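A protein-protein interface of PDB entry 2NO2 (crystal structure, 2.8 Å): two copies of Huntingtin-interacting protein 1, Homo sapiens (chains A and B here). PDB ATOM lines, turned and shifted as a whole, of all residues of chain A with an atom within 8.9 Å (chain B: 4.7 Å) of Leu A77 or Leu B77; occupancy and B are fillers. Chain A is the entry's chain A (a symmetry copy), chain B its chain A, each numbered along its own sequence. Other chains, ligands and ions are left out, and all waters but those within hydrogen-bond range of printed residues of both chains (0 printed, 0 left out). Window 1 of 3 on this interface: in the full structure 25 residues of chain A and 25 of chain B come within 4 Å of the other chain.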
ATOM      1  N   LEU A  70       4.082  11.216  12.995  1.00  0.00           N
ATOM      2  CA  LEU A  70       5.214  11.986  12.491  1.00  0.00           C
ATOM      3  C   LEU A  70       4.874  13.455  12.382  1.00  0.00           C
ATOM      4  O   LEU A  70       5.710  14.309  12.652  1.00  0.00           O
ATOM      5  CB  LEU A  70       5.634  11.510  11.113  1.00  0.00           C
ATOM      6  CG  LEU A  70       6.846  10.594  11.079  1.00  0.00           C
ATOM      7  CD1 LEU A  70       7.145  10.250   9.626  1.00  0.00           C
ATOM      8  CD2 LEU A  70       8.036  11.268  11.751  1.00  0.00           C
ATOM      9  N   GLN A  71       3.649  13.752  11.972  1.00  0.00           N
ATOM     10  CA  GLN A  71       3.244  15.137  11.831  1.00  0.00           C
ATOM     11  C   GLN A  71       3.168  15.817  13.193  1.00  0.00           C
ATOM     12  O   GLN A  71       3.493  16.996  13.332  1.00  0.00           O
ATOM     13  CB  GLN A  71       1.901  15.219  11.130  1.00  0.00           C
ATOM     14  CG  GLN A  71       1.535  16.612  10.738  1.00  0.00           C
ATOM     15  CD  GLN A  71       0.272  16.641   9.936  1.00  0.00           C
ATOM     16  OE1 GLN A  71      -0.780  16.215  10.407  1.00  0.00           O
ATOM     17  NE2 GLN A  71       0.359  17.135   8.707  1.00  0.00           N
ATOM     18  N   VAL A  72       2.752  15.073  14.209  1.00  0.00           N
ATOM     19  CA  VAL A  72       2.658  15.654  15.538  1.00  0.00           C
ATOM     20  C   VAL A  72       4.037  15.950  16.084  1.00  0.00           C
ATOM     21  O   VAL A  72       4.235  16.992  16.702  1.00  0.00           O
ATOM     22  CB  VAL A  72       1.916  14.735  16.519  1.00  0.00           C
ATOM     23  CG1 VAL A  72       2.025  15.291  17.920  1.00  0.00           C
ATOM     24  CG2 VAL A  72       0.449  14.621  16.117  1.00  0.00           C
ATOM     25  N   LEU A  73       4.994  15.052  15.873  1.00  0.00           N
ATOM     26  CA  LEU A  73       6.345  15.324  16.365  1.00  0.00           C
ATOM     27  C   LEU A  73       6.968  16.519  15.646  1.00  0.00           C
ATOM     28  O   LEU A  73       7.656  17.331  16.280  1.00  0.00           O
ATOM     29  CB  LEU A  73       7.245  14.104  16.222  1.00  0.00           C
ATOM     30  CG  LEU A  73       6.792  12.942  17.104  1.00  0.00           C
ATOM     31  CD1 LEU A  73       7.988  12.036  17.387  1.00  0.00           C
ATOM     32  CD2 LEU A  73       6.226  13.466  18.408  1.00  0.00           C
ATOM     33  N   GLN A  74       6.718  16.635  14.338  1.00  0.00           N
ATOM     34  CA  GLN A  74       7.244  17.758  13.578  1.00  0.00           C
ATOM     35  C   GLN A  74       6.794  19.056  14.245  1.00  0.00           C
ATOM     36  O   GLN A  74       7.536  20.048  14.271  1.00  0.00           O
ATOM     37  CB  GLN A  74       6.777  17.715  12.128  1.00  0.00           C
ATOM     38  CG  GLN A  74       7.888  17.326  11.182  1.00  0.00           C
ATOM     39  CD  GLN A  74       7.482  17.440   9.737  1.00  0.00           C
ATOM     40  OE1 GLN A  74       6.555  16.767   9.284  1.00  0.00           O
ATOM     41  NE2 GLN A  74       8.175  18.297   8.996  1.00  0.00           N
ATOM     42  N   GLY A  75       5.585  19.038  14.808  1.00  0.00           N
ATOM     43  CA  GLY A  75       5.071  20.207  15.505  1.00  0.00           C
ATOM     44  C   GLY A  75       5.724  20.395  16.872  1.00  0.00           C
ATOM     45  O   GLY A  75       6.045  21.518  17.271  1.00  0.00           O
ATOM     46  N   SER A  76       5.916  19.303  17.608  1.00  0.00           N
ATOM     47  CA  SER A  76       6.549  19.400  18.916  1.00  0.00           C
ATOM     48  C   SER A  76       7.964  19.944  18.756  1.00  0.00           C
ATOM     49  O   SER A  76       8.421  20.755  19.565  1.00  0.00           O
ATOM     50  CB  SER A  76       6.576  18.036  19.588  1.00  0.00           C
ATOM     51  OG  SER A  76       5.255  17.637  19.889  1.00  0.00           O
ATOM     52  N   LEU A  77       8.656  19.499  17.708  1.00  0.00           N
ATOM     53  CA  LEU A  77       9.999  19.994  17.442  1.00  0.00           C
ATOM     54  C   LEU A  77       9.888  21.497  17.152  1.00  0.00           C
ATOM     55  O   LEU A  77      10.642  22.307  17.701  1.00  0.00           O
ATOM     56  CB  LEU A  77      10.610  19.263  16.253  1.00  0.00           C
ATOM     57  CG  LEU A  77      12.020  18.722  16.510  1.00  0.00           C
ATOM     58  CD1 LEU A  77      12.926  19.860  16.965  1.00  0.00           C
ATOM     59  CD2 LEU A  77      11.989  17.641  17.572  1.00  0.00           C
ATOM     60  N   GLU A  78       8.924  21.857  16.303  1.00  0.00           N
ATOM     61  CA  GLU A  78       8.643  23.253  15.944  1.00  0.00           C
ATOM     62  C   GLU A  78       8.471  24.132  17.204  1.00  0.00           C
ATOM     63  O   GLU A  78       9.106  25.182  17.344  1.00  0.00           O
ATOM     64  CB  GLU A  78       7.361  23.306  15.106  1.00  0.00           C
ATOM     65  CG  GLU A  78       7.069  24.649  14.484  1.00  0.00           C
ATOM     66  CD  GLU A  78       8.105  25.024  13.454  1.00  0.00           C
ATOM     67  OE1 GLU A  78       8.307  24.226  12.515  1.00  0.00           O
ATOM     68  OE2 GLU A  78       8.714  26.108  13.583  1.00  0.00           O
ATOM     69  N   THR A  79       7.606  23.698  18.119  1.00  0.00           N
ATOM     70  CA  THR A  79       7.365  24.438  19.358  1.00  0.00           C
ATOM     71  C   THR A  79       8.605  24.444  20.249  1.00  0.00           C
ATOM     72  O   THR A  79       9.051  25.502  20.703  1.00  0.00           O
ATOM     73  CB  THR A  79       6.182  23.834  20.157  1.00  0.00           C
ATOM     74  OG1 THR A  79       4.952  24.149  19.496  1.00  0.00           O
ATOM     75  CG2 THR A  79       6.148  24.389  21.575  1.00  0.00           C
ATOM     76  N   SER A  80       9.157  23.264  20.510  1.00  0.00           N
ATOM     77  CA  SER A  80      10.347  23.191  21.340  1.00  0.00           C
ATOM     78  C   SER A  80      11.374  24.168  20.763  1.00  0.00           C
ATOM     79  O   SER A  80      11.950  24.977  21.489  1.00  0.00           O
ATOM     80  CB  SER A  80      10.907  21.765  21.360  1.00  0.00           C
ATOM     81  OG  SER A  80      11.934  21.631  22.336  1.00  0.00           O
ATOM     82  N   ALA A  81      11.585  24.114  19.453  1.00  0.00           N
ATOM     83  CA  ALA A  81      12.538  25.018  18.820  1.00  0.00           C
ATOM     84  C   ALA A  81      12.228  26.461  19.192  1.00  0.00           C
ATOM     85  O   ALA A  81      13.109  27.200  19.666  1.00  0.00           O
ATOM     86  CB  ALA A  81      12.490  24.863  17.338  1.00  0.00           C
ATOM     87  N   GLN A  82      10.977  26.866  18.969  1.00  0.00           N
ATOM     88  CA  GLN A  82      10.568  28.220  19.315  1.00  0.00           C
ATOM     89  C   GLN A  82      10.865  28.502  20.794  1.00  0.00           C
ATOM     90  O   GLN A  82      11.228  29.626  21.156  1.00  0.00           O
ATOM     91  CB  GLN A  82       9.078  28.421  19.034  1.00  0.00           C
ATOM     92  CG  GLN A  82       8.592  29.818  19.382  1.00  0.00           C
ATOM     93  CD  GLN A  82       9.402  30.907  18.695  1.00  0.00           C
ATOM     94  OE1 GLN A  82       9.432  32.051  19.148  1.00  0.00           O
ATOM     95  NE2 GLN A  82      10.053  30.558  17.590  1.00  0.00           N
ATOM     96  N   SER A  83      10.736  27.484  21.645  1.00  0.00           N
ATOM     97  CA  SER A  83      10.994  27.674  23.062  1.00  0.00           C
ATOM     98  C   SER A  83      12.457  27.924  23.346  1.00  0.00           C
ATOM     99  O   SER A  83      12.795  28.801  24.150  1.00  0.00           O
ATOM    100  CB  SER A  83      10.540  26.476  23.873  1.00  0.00           C
ATOM    101  OG  SER A  83      10.685  26.759  25.252  1.00  0.00           O
ATOM    102  N   GLU A  84      13.334  27.155  22.710  1.00  0.00           N
ATOM    103  CA  GLU A  84      14.761  27.357  22.916  1.00  0.00           C
ATOM    104  C   GLU A  84      15.127  28.767  22.518  1.00  0.00           C
ATOM    105  O   GLU A  84      15.980  29.386  23.151  1.00  0.00           O
ATOM    106  CB  GLU A  84      15.578  26.393  22.094  1.00  0.00           C
ATOM    107  CG  GLU A  84      15.424  25.005  22.563  1.00  0.00           C
ATOM    108  CD  GLU A  84      16.616  24.166  22.227  1.00  0.00           C
ATOM    109  OE1 GLU A  84      17.741  24.546  22.624  1.00  0.00           O
ATOM    110  OE2 GLU A  84      16.422  23.121  21.574  1.00  0.00           O
ATOM    111  N   ALA A  85      14.487  29.276  21.467  1.00  0.00           N
ATOM    112  CA  ALA A  85      14.739  30.648  21.028  1.00  0.00           C
ATOM    113  C   ALA A  85      14.469  31.613  22.183  1.00  0.00           C
ATOM    114  O   ALA A  85      15.334  32.414  22.563  1.00  0.00           O
ATOM    115  CB  ALA A  85      13.850  30.998  19.859  1.00  0.00           C
ATOM    116  N   LEU B  73      12.919  11.645  14.950  1.00  0.00           N
ATOM    117  CA  LEU B  73      12.317  12.804  15.610  1.00  0.00           C
ATOM    118  C   LEU B  73      12.207  12.590  17.119  1.00  0.00           C
ATOM    119  O   LEU B  73      12.437  13.529  17.894  1.00  0.00           O
ATOM    120  CB  LEU B  73      10.946  13.125  15.030  1.00  0.00           C
ATOM    121  CG  LEU B  73      11.024  13.570  13.571  1.00  0.00           C
ATOM    122  CD1 LEU B  73       9.800  14.422  13.244  1.00  0.00           C
ATOM    123  CD2 LEU B  73      12.286  14.375  13.336  1.00  0.00           C
ATOM    124  N   GLN B  74      11.876  11.363  17.533  1.00  0.00           N
ATOM    125  CA  GLN B  74      11.779  11.059  18.952  1.00  0.00           C
ATOM    126  C   GLN B  74      13.100  11.425  19.624  1.00  0.00           C
ATOM    127  O   GLN B  74      13.122  11.891  20.772  1.00  0.00           O
ATOM    128  CB  GLN B  74      11.453   9.588  19.183  1.00  0.00           C
ATOM    129  CG  GLN B  74      10.033   9.385  19.653  1.00  0.00           C
ATOM    130  CD  GLN B  74       9.751   7.958  20.041  1.00  0.00           C
ATOM    131  OE1 GLN B  74       9.848   7.047  19.219  1.00  0.00           O
ATOM    132  NE2 GLN B  74       9.398   7.750  21.304  1.00  0.00           N
ATOM    133  N   GLY B  75      14.201  11.236  18.895  1.00  0.00           N
ATOM    134  CA  GLY B  75      15.512  11.587  19.422  1.00  0.00           C
ATOM    135  C   GLY B  75      15.747  13.096  19.420  1.00  0.00           C
ATOM    136  O   GLY B  75      16.304  13.651  20.371  1.00  0.00           O
ATOM    137  N   SER B  76      15.337  13.772  18.350  1.00  0.00           N
ATOM    138  CA  SER B  76      15.511  15.217  18.282  1.00  0.00           C
ATOM    139  C   SER B  76      14.726  15.876  19.410  1.00  0.00           C
ATOM    140  O   SER B  76      15.196  16.836  20.027  1.00  0.00           O
ATOM    141  CB  SER B  76      15.044  15.739  16.933  1.00  0.00           C
ATOM    142  OG  SER B  76      15.902  15.256  15.922  1.00  0.00           O
ATOM    143  N   LEU B  77      13.530  15.357  19.683  1.00  0.00           N
ATOM    144  CA  LEU B  77      12.722  15.886  20.773  1.00  0.00           C
ATOM    145  C   LEU B  77      13.494  15.644  22.078  1.00  0.00           C
ATOM    146  O   LEU B  77      13.637  16.548  22.908  1.00  0.00           O
ATOM    147  CB  LEU B  77      11.366  15.194  20.816  1.00  0.00           C
ATOM    148  CG  LEU B  77      10.176  16.156  20.898  1.00  0.00           C
ATOM    149  CD1 LEU B  77      10.349  17.076  22.100  1.00  0.00           C
ATOM    150  CD2 LEU B  77      10.075  16.984  19.633  1.00  0.00           C
ATOM    151  N   GLU B  78      14.007  14.423  22.233  1.00  0.00           N
ATOM    152  CA  GLU B  78      14.811  14.025  23.396  1.00  0.00           C
ATOM    153  C   GLU B  78      15.965  15.023  23.646  1.00  0.00           C
ATOM    154  O   GLU B  78      16.144  15.528  24.759  1.00  0.00           O
ATOM    155  CB  GLU B  78      15.388  12.627  23.151  1.00  0.00           C
ATOM    156  CG  GLU B  78      16.055  12.002  24.351  1.00  0.00           C
ATOM    157  CD  GLU B  78      15.068  11.719  25.455  1.00  0.00           C
ATOM    158  OE1 GLU B  78      14.077  11.010  25.181  1.00  0.00           O
ATOM    159  OE2 GLU B  78      15.280  12.203  26.588  1.00  0.00           O
ATOM    160  N   THR B  79      16.748  15.300  22.606  1.00  0.00           N
ATOM    161  CA  THR B  79      17.867  16.236  22.715  1.00  0.00           C
ATOM    162  C   THR B  79      17.375  17.659  22.974  1.00  0.00           C
ATOM    163  O   THR B  79      17.831  18.324  23.908  1.00  0.00           O
ATOM    164  CB  THR B  79      18.733  16.237  21.431  1.00  0.00           C
ATOM    165  OG1 THR B  79      19.494  15.026  21.371  1.00  0.00           O
ATOM    166  CG2 THR B  79      19.682  17.428  21.418  1.00  0.00           C
ATOM    167  N   SER B  80      16.452  18.130  22.143  1.00  0.00           N
ATOM    168  CA  SER B  80      15.926  19.471  22.333  1.00  0.00           C
ATOM    169  C   SER B  80      15.471  19.587  23.790  1.00  0.00           C
ATOM    170  O   SER B  80      15.818  20.541  24.484  1.00  0.00           O
ATOM    171  CB  SER B  80      14.757  19.735  21.378  1.00  0.00           C
ATOM    172  OG  SER B  80      14.378  21.106  21.398  1.00  0.00           O
ATOM    173  N   ALA B  81      14.716  18.602  24.264  1.00  0.00           N
ATOM    174  CA  ALA B  81      14.250  18.628  25.646  1.00  0.00           C
ATOM    175  C   ALA B  81      15.421  18.829  26.597  1.00  0.00           C
ATOM    176  O   ALA B  81      15.402  19.736  27.448  1.00  0.00           O
ATOM    177  CB  ALA B  81      13.550  17.354  25.978  1.00  0.00           C
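OG of Ser B80 is in hydrogen-bond range of OG of Ser A80 (2.7 Å). OE2 of Glu A84 lies within hydrogen-bond range of OG of Ser B80 (2.9 Å).
The side-chain hydroxyl (OG) of Ser A76 sits at hydrogen-bond distance from the backbone carbonyl oxygen (O) of Val A72 (3.4 Å).
Leu A70 touches Leu B73. Leu B73 touches Leu A73 (CB to CD1, 3.9 Å). N of Gln B74 touches CD1 of Leu A73, 3.9 Å away. Gln A74 touches Leu B73 (N to CD1, 3.9 Å). Ser A76 touches Leu B77 (CB to CD2, 3.7 Å). CB of Ser B76 touches CD2 of Leu A77, 3.7 Å away. CD2 of Leu A77 touches CD2 of Leu B77, at 2.9 Å.
Printed residues of chain B within 4 Å of Leu A70: Leu B73. Of chain B, only Ser B76 (3.7 Å) and Leu B77 (2.9 Å) come within 4 Å of Leu A77. Glu A78 touches none of the printed residues of chain B. Printed residues of chain B within 4 Å of Ser A80: Ser B80 (2.7 Å). Ala A81 touches none of the printed residues of chain B. Gly B75 touches none of the printed residues of chain A. Of chain A, only Leu A77 (3.7 Å) comes within 4 Å of Ser B76. Of chain A, only Ser A76 and Leu A77 come within 4 Å of Leu B77. Of chain A, only Ser A80 (2.7 Å) and Glu A84 (2.9 Å) come within 4 Å of Ser B80. The nearest residue of chain B that does not touch Leu A77 is Leu B73 (4.1 Å). The nearest printed residue of chain B that does not touch Leu A70 is Gln B74 (6.9 Å).
Of the 16 printed residues of chain A, 7 touch a printed residue of chain B. Printed residues of chain A that touch a printed residue of chain B: Leu A70, Leu A73, Gln A74, Ser A76, Leu A77, Ser A80 and Glu A84. Hydrophobic or aromatic side chains of chain A that line the printed part of chain B: Leu A70, Leu A73 and Leu A77. Of the 9 printed residues of chain B, 5 touch a printed residue of chain A. Among the printed residues, no Asp or Glu carboxylate lies within 4 Å of a Lys or Arg side-chain nitrogen of the other chain.
Leu A73 touches Gln B74, and with the chains exchanged Gln A74 touches Leu B73. Ser A76 touches Leu B77, and with the chains exchanged Leu A77 touches Ser B76. Leu B77 touches its own counterpart, Leu A77. Ser A80 touches its own counterpart, Ser B80. 9 positions are printed for both chains. Of the 9 pairs that touch across the chains among the printed residues, 7 have their exchanged pair printed and touching as well.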
